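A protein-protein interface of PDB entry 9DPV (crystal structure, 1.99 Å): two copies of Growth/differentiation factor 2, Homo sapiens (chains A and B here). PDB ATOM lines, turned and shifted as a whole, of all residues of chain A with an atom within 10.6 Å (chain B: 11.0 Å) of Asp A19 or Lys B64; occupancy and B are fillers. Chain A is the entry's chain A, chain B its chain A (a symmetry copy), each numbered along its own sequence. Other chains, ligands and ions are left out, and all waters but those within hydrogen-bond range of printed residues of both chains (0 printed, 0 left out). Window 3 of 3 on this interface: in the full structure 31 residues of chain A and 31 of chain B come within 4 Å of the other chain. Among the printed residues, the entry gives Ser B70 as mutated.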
ATOM      1  N   LEU A  13      -8.562  19.739   2.026  1.00  0.00           N
ATOM      2  CA  LEU A  13      -9.460  20.331   3.003  1.00  0.00           C
ATOM      3  C   LEU A  13      -8.687  20.492   4.307  1.00  0.00           C
ATOM      4  O   LEU A  13      -8.450  19.520   5.022  1.00  0.00           O
ATOM      5  CB  LEU A  13     -10.727  19.499   3.231  1.00  0.00           C
ATOM      6  CG  LEU A  13     -11.694  20.080   4.314  1.00  0.00           C
ATOM      7  CD1 LEU A  13     -12.282  21.386   3.874  1.00  0.00           C
ATOM      8  CD2 LEU A  13     -12.822  19.104   4.645  1.00  0.00           C
ATOM      9  N   ARG A  14      -8.282  21.731   4.583  1.00  0.00           N
ATOM     10  CA  ARG A  14      -7.571  22.051   5.805  1.00  0.00           C
ATOM     11  C   ARG A  14      -8.581  22.408   6.892  1.00  0.00           C
ATOM     12  O   ARG A  14      -9.371  23.330   6.715  1.00  0.00           O
ATOM     13  CB  ARG A  14      -6.592  23.194   5.562  1.00  0.00           C
ATOM     14  CG  ARG A  14      -5.577  23.310   6.674  1.00  0.00           C
ATOM     15  CD  ARG A  14      -4.393  24.172   6.301  1.00  0.00           C
ATOM     16  NE  ARG A  14      -3.395  24.178   7.362  1.00  0.00           N
ATOM     17  CZ  ARG A  14      -2.685  23.119   7.732  1.00  0.00           C
ATOM     18  NH1 ARG A  14      -2.650  22.018   6.998  1.00  0.00           N
ATOM     19  NH2 ARG A  14      -1.980  23.171   8.861  1.00  0.00           N
ATOM     20  N   VAL A  15      -8.544  21.654   7.997  1.00  0.00           N
ATOM     21  CA  VAL A  15      -9.480  21.797   9.100  1.00  0.00           C
ATOM     22  C   VAL A  15      -8.805  22.469  10.315  1.00  0.00           C
ATOM     23  O   VAL A  15      -7.824  21.908  10.834  1.00  0.00           O
ATOM     24  CB  VAL A  15     -10.043  20.423   9.492  1.00  0.00           C
ATOM     25  CG1 VAL A  15     -10.841  20.501  10.796  1.00  0.00           C
ATOM     26  CG2 VAL A  15     -10.869  19.823   8.360  1.00  0.00           C
ATOM     27  N   ASN A  16      -9.402  23.553  10.822  1.00  0.00           N
ATOM     28  CA  ASN A  16      -9.074  24.189  12.135  1.00  0.00           C
ATOM     29  C   ASN A  16      -9.981  23.650  13.250  1.00  0.00           C
ATOM     30  O   ASN A  16     -11.202  23.800  13.129  1.00  0.00           O
ATOM     31  CB  ASN A  16      -9.121  25.707  11.997  1.00  0.00           C
ATOM     32  CG  ASN A  16      -8.625  26.438  13.224  1.00  0.00           C
ATOM     33  OD1 ASN A  16      -9.222  26.338  14.290  1.00  0.00           O
ATOM     34  ND2 ASN A  16      -7.544  27.182  13.079  1.00  0.00           N
ATOM     35  N   PHE A  17      -9.409  23.049  14.293  1.00  0.00           N
ATOM     36  CA  PHE A  17     -10.158  22.446  15.381  1.00  0.00           C
ATOM     37  C   PHE A  17     -10.978  23.450  16.193  1.00  0.00           C
ATOM     38  O   PHE A  17     -12.044  23.107  16.689  1.00  0.00           O
ATOM     39  CB  PHE A  17      -9.196  21.693  16.300  1.00  0.00           C
ATOM     40  CG  PHE A  17      -8.655  20.429  15.685  1.00  0.00           C
ATOM     41  CD1 PHE A  17      -9.511  19.418  15.271  1.00  0.00           C
ATOM     42  CD2 PHE A  17      -7.296  20.257  15.494  1.00  0.00           C
ATOM     43  CE1 PHE A  17      -9.015  18.257  14.702  1.00  0.00           C
ATOM     44  CE2 PHE A  17      -6.805  19.092  14.920  1.00  0.00           C
ATOM     45  CZ  PHE A  17      -7.665  18.096  14.541  1.00  0.00           C
ATOM     46  N   GLU A  18     -10.472  24.678  16.342  1.00  0.00           N
ATOM     47  CA  GLU A  18     -11.255  25.751  16.933  1.00  0.00           C
ATOM     48  C   GLU A  18     -12.528  26.009  16.133  1.00  0.00           C
ATOM     49  O   GLU A  18     -13.608  26.140  16.714  1.00  0.00           O
ATOM     50  CB  GLU A  18     -10.418  27.037  17.073  1.00  0.00           C
ATOM     51  CG  GLU A  18     -11.167  28.150  17.787  1.00  0.00           C
ATOM     52  CD  GLU A  18     -10.341  29.353  18.199  1.00  0.00           C
ATOM     53  OE1 GLU A  18      -9.092  29.267  18.165  1.00  0.00           O
ATOM     54  OE2 GLU A  18     -10.949  30.390  18.551  1.00  0.00           O
ATOM     55  N   ASP A  19     -12.410  26.058  14.799  1.00  0.00           N
ATOM     56  CA  ASP A  19     -13.560  26.322  13.948  1.00  0.00           C
ATOM     57  C   ASP A  19     -14.685  25.316  14.168  1.00  0.00           C
ATOM     58  O   ASP A  19     -15.850  25.679  14.038  1.00  0.00           O
ATOM     59  CB  ASP A  19     -13.180  26.307  12.460  1.00  0.00           C
ATOM     60  CG  ASP A  19     -12.429  27.513  11.942  1.00  0.00           C
ATOM     61  OD1 ASP A  19     -12.265  28.480  12.705  1.00  0.00           O
ATOM     62  OD2 ASP A  19     -11.986  27.477  10.769  1.00  0.00           O
ATOM     63  N   ILE A  20     -14.329  24.053  14.458  1.00  0.00           N
ATOM     64  CA  ILE A  20     -15.315  22.999  14.666  1.00  0.00           C
ATOM     65  C   ILE A  20     -15.582  22.680  16.141  1.00  0.00           C
ATOM     66  O   ILE A  20     -16.248  21.693  16.445  1.00  0.00           O
ATOM     67  CB  ILE A  20     -14.920  21.708  13.904  1.00  0.00           C
ATOM     68  CG1 ILE A  20     -13.639  21.069  14.460  1.00  0.00           C
ATOM     69  CG2 ILE A  20     -14.799  21.968  12.404  1.00  0.00           C
ATOM     70  CD1 ILE A  20     -13.488  19.650  14.099  1.00  0.00           C
ATOM     71  N   GLY A  21     -15.070  23.517  17.050  1.00  0.00           N
ATOM     72  CA  GLY A  21     -15.361  23.382  18.469  1.00  0.00           C
ATOM     73  C   GLY A  21     -14.597  22.291  19.220  1.00  0.00           C
ATOM     74  O   GLY A  21     -14.992  21.918  20.326  1.00  0.00           O
ATOM     75  N   TRP A  22     -13.494  21.807  18.631  1.00  0.00           N
ATOM     76  CA  TRP A  22     -12.692  20.743  19.223  1.00  0.00           C
ATOM     77  C   TRP A  22     -11.420  21.221  19.929  1.00  0.00           C
ATOM     78  O   TRP A  22     -10.692  20.415  20.520  1.00  0.00           O
ATOM     79  CB  TRP A  22     -12.322  19.700  18.147  1.00  0.00           C
ATOM     80  CG  TRP A  22     -13.430  18.766  17.766  1.00  0.00           C
ATOM     81  CD1 TRP A  22     -14.760  18.893  18.047  1.00  0.00           C
ATOM     82  CD2 TRP A  22     -13.289  17.544  17.031  1.00  0.00           C
ATOM     83  NE1 TRP A  22     -15.461  17.826  17.516  1.00  0.00           N
ATOM     84  CE2 TRP A  22     -14.578  16.983  16.893  1.00  0.00           C
ATOM     85  CE3 TRP A  22     -12.197  16.873  16.465  1.00  0.00           C
ATOM     86  CZ2 TRP A  22     -14.797  15.781  16.221  1.00  0.00           C
ATOM     87  CZ3 TRP A  22     -12.415  15.681  15.807  1.00  0.00           C
ATOM     88  CH2 TRP A  22     -13.701  15.149  15.682  1.00  0.00           C
ATOM     89  N   ASP A  23     -11.161  22.535  19.887  1.00  0.00           N
ATOM     90  CA  ASP A  23     -10.010  23.116  20.561  1.00  0.00           C
ATOM     91  C   ASP A  23     -10.170  23.076  22.082  1.00  0.00           C
ATOM     92  O   ASP A  23      -9.211  23.297  22.813  1.00  0.00           O
ATOM     93  CB  ASP A  23      -9.800  24.564  20.098  1.00  0.00           C
ATOM     94  CG  ASP A  23     -10.931  25.479  20.502  1.00  0.00           C
ATOM     95  OD1 ASP A  23     -12.101  25.097  20.292  1.00  0.00           O
ATOM     96  OD2 ASP A  23     -10.648  26.575  21.019  1.00  0.00           O
ATOM     97  N   SER A  24     -11.392  22.806  22.548  1.00  0.00           N
ATOM     98  CA  SER A  24     -11.637  22.532  23.953  1.00  0.00           C
ATOM     99  C   SER A  24     -10.865  21.320  24.473  1.00  0.00           C
ATOM    100  O   SER A  24     -10.504  21.288  25.647  1.00  0.00           O
ATOM    101  CB  SER A  24     -13.134  22.351  24.203  1.00  0.00           C
ATOM    102  OG  SER A  24     -13.698  21.405  23.310  1.00  0.00           O
ATOM    103  N   ILE A  26      -8.565  19.213  21.993  1.00  0.00           N
ATOM    104  CA  ILE A  26      -7.327  19.097  21.236  1.00  0.00           C
ATOM    105  C   ILE A  26      -6.449  20.328  21.444  1.00  0.00           C
ATOM    106  O   ILE A  26      -6.820  21.433  21.059  1.00  0.00           O
ATOM    107  CB  ILE A  26      -7.590  18.860  19.733  1.00  0.00           C
ATOM    108  CG1 ILE A  26      -8.298  17.518  19.516  1.00  0.00           C
ATOM    109  CG2 ILE A  26      -6.280  18.943  18.930  1.00  0.00           C
ATOM    110  CD1 ILE A  26      -8.874  17.352  18.232  1.00  0.00           C
ATOM    111  N   PRO A  29      -2.443  19.368  16.911  1.00  0.00           N
ATOM    112  CA  PRO A  29      -2.151  20.638  16.254  1.00  0.00           C
ATOM    113  C   PRO A  29      -3.372  21.551  16.201  1.00  0.00           C
ATOM    114  O   PRO A  29      -4.473  21.110  16.507  1.00  0.00           O
ATOM    115  CB  PRO A  29      -1.756  20.192  14.853  1.00  0.00           C
ATOM    116  CG  PRO A  29      -2.658  18.998  14.613  1.00  0.00           C
ATOM    117  CD  PRO A  29      -2.699  18.282  15.949  1.00  0.00           C
ATOM    118  N   LYS A  30      -3.171  22.801  15.774  1.00  0.00           N
ATOM    119  CA  LYS A  30      -4.262  23.750  15.615  1.00  0.00           C
ATOM    120  C   LYS A  30      -5.079  23.491  14.349  1.00  0.00           C
ATOM    121  O   LYS A  30      -6.276  23.776  14.316  1.00  0.00           O
ATOM    122  CB  LYS A  30      -3.712  25.181  15.606  1.00  0.00           C
ATOM    123  CG  LYS A  30      -3.159  25.637  16.971  1.00  0.00           C
ATOM    124  CD  LYS A  30      -4.232  25.686  18.062  1.00  0.00           C
ATOM    125  CE  LYS A  30      -3.781  26.382  19.333  1.00  0.00           C
ATOM    126  NZ  LYS A  30      -4.905  26.537  20.304  1.00  0.00           N
ATOM    127  N   GLU A  31      -4.411  22.967  13.315  1.00  0.00           N
ATOM    128  CA  GLU A  31      -5.024  22.693  12.024  1.00  0.00           C
ATOM    129  C   GLU A  31      -4.428  21.416  11.442  1.00  0.00           C
ATOM    130  O   GLU A  31      -3.309  21.044  11.782  1.00  0.00           O
ATOM    131  CB  GLU A  31      -4.768  23.832  11.020  1.00  0.00           C
ATOM    132  CG  GLU A  31      -5.280  25.194  11.436  1.00  0.00           C
ATOM    133  CD  GLU A  31      -5.272  26.243  10.337  1.00  0.00           C
ATOM    134  OE1 GLU A  31      -4.910  25.908   9.187  1.00  0.00           O
ATOM    135  OE2 GLU A  31      -5.628  27.406  10.631  1.00  0.00           O
ATOM    136  N   TYR A  32      -5.167  20.759  10.543  1.00  0.00           N
ATOM    137  CA  TYR A  32      -4.607  19.629   9.822  1.00  0.00           C
ATOM    138  C   TYR A  32      -5.276  19.489   8.459  1.00  0.00           C
ATOM    139  O   TYR A  32      -6.310  20.097   8.202  1.00  0.00           O
ATOM    140  CB  TYR A  32      -4.713  18.332  10.645  1.00  0.00           C
ATOM    141  CG  TYR A  32      -6.026  17.595  10.528  1.00  0.00           C
ATOM    142  CD1 TYR A  32      -7.189  18.122  11.061  1.00  0.00           C
ATOM    143  CD2 TYR A  32      -6.105  16.368   9.877  1.00  0.00           C
ATOM    144  CE1 TYR A  32      -8.397  17.445  10.970  1.00  0.00           C
ATOM    145  CE2 TYR A  32      -7.308  15.679   9.783  1.00  0.00           C
ATOM    146  CZ  TYR A  32      -8.453  16.219  10.335  1.00  0.00           C
ATOM    147  OH  TYR A  32      -9.665  15.573  10.252  1.00  0.00           O
ATOM    148  N   PHE B  43     -26.156  17.073  12.543  1.00  0.00           N
ATOM    149  CA  PHE B  43     -26.262  16.954  13.987  1.00  0.00           C
ATOM    150  C   PHE B  43     -27.652  17.356  14.462  1.00  0.00           C
ATOM    151  O   PHE B  43     -28.253  18.280  13.920  1.00  0.00           O
ATOM    152  CB  PHE B  43     -25.201  17.802  14.679  1.00  0.00           C
ATOM    153  CG  PHE B  43     -23.822  17.305  14.335  1.00  0.00           C
ATOM    154  CD1 PHE B  43     -23.362  16.096  14.825  1.00  0.00           C
ATOM    155  CD2 PHE B  43     -23.009  18.015  13.470  1.00  0.00           C
ATOM    156  CE1 PHE B  43     -22.092  15.633  14.502  1.00  0.00           C
ATOM    157  CE2 PHE B  43     -21.743  17.542  13.136  1.00  0.00           C
ATOM    158  CZ  PHE B  43     -21.295  16.354  13.651  1.00  0.00           C
ATOM    159  N   ILE B  56     -17.774  13.243  10.646  1.00  0.00           N
ATOM    160  CA  ILE B  56     -18.123  14.173  11.706  1.00  0.00           C
ATOM    161  C   ILE B  56     -17.438  15.520  11.487  1.00  0.00           C
ATOM    162  O   ILE B  56     -18.085  16.565  11.514  1.00  0.00           O
ATOM    163  CB  ILE B  56     -17.780  13.526  13.079  1.00  0.00           C
ATOM    164  CG1 ILE B  56     -18.693  12.303  13.323  1.00  0.00           C
ATOM    165  CG2 ILE B  56     -17.879  14.511  14.195  1.00  0.00           C
ATOM    166  CD1 ILE B  56     -18.291  11.422  14.486  1.00  0.00           C
ATOM    167  N   VAL B  57     -16.121  15.485  11.264  1.00  0.00           N
ATOM    168  CA  VAL B  57     -15.348  16.693  11.015  1.00  0.00           C
ATOM    169  C   VAL B  57     -15.849  17.464   9.796  1.00  0.00           C
ATOM    170  O   VAL B  57     -16.019  18.677   9.840  1.00  0.00           O
ATOM    171  CB  VAL B  57     -13.867  16.327  10.869  1.00  0.00           C
ATOM    172  CG1 VAL B  57     -13.074  17.437  10.198  1.00  0.00           C
ATOM    173  CG2 VAL B  57     -13.279  15.970  12.221  1.00  0.00           C
ATOM    174  N   GLN B  58     -16.093  16.747   8.699  1.00  0.00           N
ATOM    175  CA  GLN B  58     -16.562  17.401   7.492  1.00  0.00           C
ATOM    176  C   GLN B  58     -17.929  18.049   7.695  1.00  0.00           C
ATOM    177  O   GLN B  58     -18.163  19.166   7.244  1.00  0.00           O
ATOM    178  CB  GLN B  58     -16.584  16.401   6.316  1.00  0.00           C
ATOM    179  CG  GLN B  58     -16.930  17.115   5.036  1.00  0.00           C
ATOM    180  CD  GLN B  58     -16.676  16.312   3.809  1.00  0.00           C
ATOM    181  OE1 GLN B  58     -15.807  15.454   3.775  1.00  0.00           O
ATOM    182  NE2 GLN B  58     -17.446  16.612   2.775  1.00  0.00           N
ATOM    183  N   THR B  59     -18.824  17.361   8.408  1.00  0.00           N
ATOM    184  CA  THR B  59     -20.134  17.914   8.719  1.00  0.00           C
ATOM    185  C   THR B  59     -20.041  19.213   9.518  1.00  0.00           C
ATOM    186  O   THR B  59     -20.782  20.160   9.252  1.00  0.00           O
ATOM    187  CB  THR B  59     -20.977  16.862   9.432  1.00  0.00           C
ATOM    188  OG1 THR B  59     -21.019  15.682   8.611  1.00  0.00           O
ATOM    189  CG2 THR B  59     -22.403  17.359   9.734  1.00  0.00           C
ATOM    190  N   LEU B  60     -19.121  19.256  10.490  1.00  0.00           N
ATOM    191  CA  LEU B  60     -18.881  20.465  11.262  1.00  0.00           C
ATOM    192  C   LEU B  60     -18.284  21.584  10.412  1.00  0.00           C
ATOM    193  O   LEU B  60     -18.663  22.742  10.551  1.00  0.00           O
ATOM    194  CB  LEU B  60     -17.945  20.155  12.443  1.00  0.00           C
ATOM    195  CG  LEU B  60     -18.548  19.264  13.542  1.00  0.00           C
ATOM    196  CD1 LEU B  60     -17.487  18.845  14.551  1.00  0.00           C
ATOM    197  CD2 LEU B  60     -19.677  19.967  14.250  1.00  0.00           C
ATOM    198  N   VAL B  61     -17.351  21.233   9.520  1.00  0.00           N
ATOM    199  CA  VAL B  61     -16.772  22.220   8.622  1.00  0.00           C
ATOM    200  C   VAL B  61     -17.835  22.769   7.673  1.00  0.00           C
ATOM    201  O   VAL B  61     -17.874  23.972   7.419  1.00  0.00           O
ATOM    202  CB  VAL B  61     -15.568  21.646   7.835  1.00  0.00           C
ATOM    203  CG1 VAL B  61     -15.065  22.652   6.806  1.00  0.00           C
ATOM    204  CG2 VAL B  61     -14.454  21.231   8.771  1.00  0.00           C
ATOM    205  N   HIS B  62     -18.684  21.882   7.146  1.00  0.00           N
ATOM    206  CA  HIS B  62     -19.807  22.301   6.320  1.00  0.00           C
ATOM    207  C   HIS B  62     -20.688  23.327   7.035  1.00  0.00           C
ATOM    208  O   HIS B  62     -21.083  24.335   6.448  1.00  0.00           O
ATOM    209  CB  HIS B  62     -20.665  21.105   5.898  1.00  0.00           C
ATOM    210  CG  HIS B  62     -21.952  21.522   5.251  1.00  0.00           C
ATOM    211  ND1 HIS B  62     -21.993  21.978   3.941  1.00  0.00           N
ATOM    212  CD2 HIS B  62     -23.201  21.567   5.762  1.00  0.00           C
ATOM    213  CE1 HIS B  62     -23.263  22.280   3.695  1.00  0.00           C
ATOM    214  NE2 HIS B  62     -24.027  22.046   4.765  1.00  0.00           N
ATOM    215  N   LEU B  63     -20.980  23.092   8.319  1.00  0.00           N
ATOM    216  CA  LEU B  63     -21.813  24.032   9.062  1.00  0.00           C
ATOM    217  C   LEU B  63     -21.191  25.421   9.088  1.00  0.00           C
ATOM    218  O   LEU B  63     -21.887  26.419   8.926  1.00  0.00           O
ATOM    219  CB  LEU B  63     -22.054  23.562  10.497  1.00  0.00           C
ATOM    220  CG  LEU B  63     -22.991  22.382  10.688  1.00  0.00           C
ATOM    221  CD1 LEU B  63     -23.232  22.132  12.160  1.00  0.00           C
ATOM    222  CD2 LEU B  63     -24.326  22.598   9.976  1.00  0.00           C
ATOM    223  N   LYS B  64     -19.873  25.479   9.300  1.00  0.00           N
ATOM    224  CA  LYS B  64     -19.177  26.749   9.395  1.00  0.00           C
ATOM    225  C   LYS B  64     -18.981  27.393   8.025  1.00  0.00           C
ATOM    226  O   LYS B  64     -19.008  28.613   7.918  1.00  0.00           O
ATOM    227  CB  LYS B  64     -17.821  26.555  10.096  1.00  0.00           C
ATOM    228  CG  LYS B  64     -17.232  27.821  10.712  1.00  0.00           C
ATOM    229  CD  LYS B  64     -17.972  28.276  11.973  1.00  0.00           C
ATOM    230  CE  LYS B  64     -17.429  29.564  12.555  1.00  0.00           C
ATOM    231  NZ  LYS B  64     -16.121  29.362  13.230  1.00  0.00           N
ATOM    232  N   PHE B  65     -18.800  26.564   6.986  1.00  0.00           N
ATOM    233  CA  PHE B  65     -18.489  27.040   5.646  1.00  0.00           C
ATOM    234  C   PHE B  65     -19.361  26.354   4.596  1.00  0.00           C
ATOM    235  O   PHE B  65     -18.849  25.616   3.754  1.00  0.00           O
ATOM    236  CB  PHE B  65     -17.007  26.763   5.333  1.00  0.00           C
ATOM    237  CG  PHE B  65     -16.033  27.412   6.274  1.00  0.00           C
ATOM    238  CD1 PHE B  65     -15.702  28.748   6.142  1.00  0.00           C
ATOM    239  CD2 PHE B  65     -15.457  26.694   7.304  1.00  0.00           C
ATOM    240  CE1 PHE B  65     -14.806  29.347   7.019  1.00  0.00           C
ATOM    241  CE2 PHE B  65     -14.561  27.296   8.178  1.00  0.00           C
ATOM    242  CZ  PHE B  65     -14.239  28.616   8.031  1.00  0.00           C
ATOM    243  N   PRO B  66     -20.698  26.559   4.611  1.00  0.00           N
ATOM    244  CA  PRO B  66     -21.611  25.765   3.800  1.00  0.00           C
ATOM    245  C   PRO B  66     -21.480  25.928   2.286  1.00  0.00           C
ATOM    246  O   PRO B  66     -21.851  25.019   1.551  1.00  0.00           O
ATOM    247  CB  PRO B  66     -22.988  26.231   4.294  1.00  0.00           C
ATOM    248  CG  PRO B  66     -22.760  27.557   4.853  1.00  0.00           C
ATOM    249  CD  PRO B  66     -21.409  27.525   5.458  1.00  0.00           C
ATOM    250  N   THR B  67     -20.993  27.082   1.813  1.00  0.00           N
ATOM    251  CA  THR B  67     -20.813  27.282   0.381  1.00  0.00           C
ATOM    252  C   THR B  67     -19.531  26.673  -0.185  1.00  0.00           C
ATOM    253  O   THR B  67     -19.397  26.565  -1.400  1.00  0.00           O
ATOM    254  CB  THR B  67     -20.851  28.759   0.019  1.00  0.00           C
ATOM    255  OG1 THR B  67     -19.729  29.406   0.610  1.00  0.00           O
ATOM    256  CG2 THR B  67     -22.144  29.423   0.461  1.00  0.00           C
ATOM    257  N   LYS B  68     -18.597  26.281   0.692  1.00  0.00           N
ATOM    258  CA  LYS B  68     -17.291  25.795   0.268  1.00  0.00           C
ATOM    259  C   LYS B  68     -17.084  24.298   0.486  1.00  0.00           C
ATOM    260  O   LYS B  68     -16.410  23.640  -0.304  1.00  0.00           O
ATOM    261  CB  LYS B  68     -16.197  26.569   1.010  1.00  0.00           C
ATOM    262  CG  LYS B  68     -16.136  28.045   0.631  1.00  0.00           C
ATOM    263  CD  LYS B  68     -14.923  28.751   1.220  1.00  0.00           C
ATOM    264  CE  LYS B  68     -14.790  30.178   0.745  1.00  0.00           C
ATOM    265  NZ  LYS B  68     -15.870  31.048   1.282  1.00  0.00           N
ATOM    266  N   VAL B  69     -17.657  23.765   1.568  1.00  0.00           N
ATOM    267  CA  VAL B  69     -17.481  22.367   1.915  1.00  0.00           C
ATOM    268  C   VAL B  69     -18.834  21.681   1.996  1.00  0.00           C
ATOM    269  O   VAL B  69     -19.756  22.198   2.620  1.00  0.00           O
ATOM    270  CB  VAL B  69     -16.734  22.230   3.245  1.00  0.00           C
ATOM    271  CG1 VAL B  69     -16.569  20.755   3.617  1.00  0.00           C
ATOM    272  CG2 VAL B  69     -15.400  22.952   3.183  1.00  0.00           C
ATOM    273  N   SER B  70     -18.933  20.496   1.396  1.00  0.00           N
ATOM    274  CA  SER B  70     -20.182  19.759   1.409  1.00  0.00           C
ATOM    275  C   SER B  70     -20.334  18.921   2.675  1.00  0.00           C
ATOM    276  O   SER B  70     -19.366  18.634   3.379  1.00  0.00           O
ATOM    277  CB  SER B  70     -20.287  18.872   0.178  1.00  0.00           C
ATOM    278  OG  SER B  70     -19.290  17.869   0.229  1.00  0.00           O
ATOM    279  N   LYS B  71     -21.569  18.540   2.927  1.00  0.00           N
ATOM    280  CA  LYS B  71     -21.839  17.674   4.082  1.00  0.00           C
ATOM    281  C   LYS B  71     -21.425  16.246   3.786  1.00  0.00           C
ATOM    282  O   LYS B  71     -21.175  15.922   2.629  1.00  0.00           O
ATOM    283  CB  LYS B  71     -23.346  17.585   4.312  1.00  0.00           C
ATOM    284  CG  LYS B  71     -24.164  18.776   3.834  1.00  0.00           C
ATOM    285  CD  LYS B  71     -24.761  18.602   2.458  1.00  0.00           C
ATOM    286  CE  LYS B  71     -24.697  19.871   1.637  1.00  0.00           C
ATOM    287  NZ  LYS B  71     -23.530  19.883   0.729  1.00  0.00           N
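The side-chain amino group (NZ) of Lys B64 lies within salt-bridge range of the side-chain carboxylate (OD1) of Asp A19 (3.99 Å).
The backbone NH (N) of Val A15 is in hydrogen-bond range of the backbone carbonyl oxygen (O) of Tyr A32, at 2.7 Å.
N of Trp A22 sits at hydrogen-bond distance from O of Phe A17 (2.8 Å).
The side-chain amide oxygen (OD1) of Asn A16 is in hydrogen-bond range of the backbone NH (N) of Asp A19 (3.2 Å).
A ring nitrogen (ND1) of His B62 sits at hydrogen-bond distance from the backbone carbonyl oxygen (O) of Val B69, 2.6 Å away.
Leu A13 touches Val B69 (CD1 to CG2, 3.6 Å).
Val B57 touches Val A15.
CG2 of Val B61 touches CG2 of Val A15, at 3.9 Å.
Phe B65 touches Asp A19.
CG2 of Ile A20 touches CB of Leu B60, at 3.6 Å.
Val B61 touches Ile A20 (CG2 to CG2, 3.7 Å).
CG2 of Ile B56 touches CZ2 of Trp A22 (3.9 Å).
Val B57 touches Trp A22.
NE1 of Trp A22 touches CD1 of Leu B60, at 3.7 Å.
CG1 of Val B57 touches OH of Tyr A32 (3.9 Å).
No residue of chain B comes within 4 Å of Asn A16.
No residue of chain B comes within 4 Å of Glu A18.
Asp A19 touches just these residues of chain B: Lys B64 (3.8 Å) and Phe B65 (3.7 Å).
Of chain B, only Leu B60 (3.6 Å) and Val B61 (3.7 Å) come within 4 Å of Ile A20.
Printed residues of chain B within 4 Å of Trp A22: Ile B56 (3.9 Å), Val B57 (3.6 Å) and Leu B60 (3.7 Å).
Printed residues of chain A within 4 Å of Val B57: Val A15 (3.7 Å), Trp A22 (3.6 Å) and Tyr A32 (3.9 Å).
Of the printed residues of chain A, Lys B64 touches Asp A19.
Phe B65 touches just one residue of chain A: Asp A19 (3.7 Å).
Of the printed residues of chain A, Val B69 touches Leu A13.
The nearest residue of chain B that does not touch Asp A19 is Leu B60 (5.4 Å).
The nearest residue of chain A that does not touch Lys B64 is Glu A18 (5.4 Å).
The nearest printed residue of chain A that does not touch Val B57 is Ile A20 (4.1 Å).
Of the 17 printed residues of chain B, 7 touch a printed residue of chain A.
Printed residues of chain A that touch a printed residue of chain B: Leu A13, Val A15, Asp A19, Ile A20, Trp A22 and Tyr A32.
Hydrophobic or aromatic side chains of chain A that line the printed part of chain B: Leu A13, Val A15, Ile A20, Trp A22 and Tyr A32.
Among the printed residues, 11 pairs touch across the chains.
No position is printed for both chains.
Of the 11 pairs that touch across the chains among the printed residues, none has its exchanged pair printed and touching as well.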
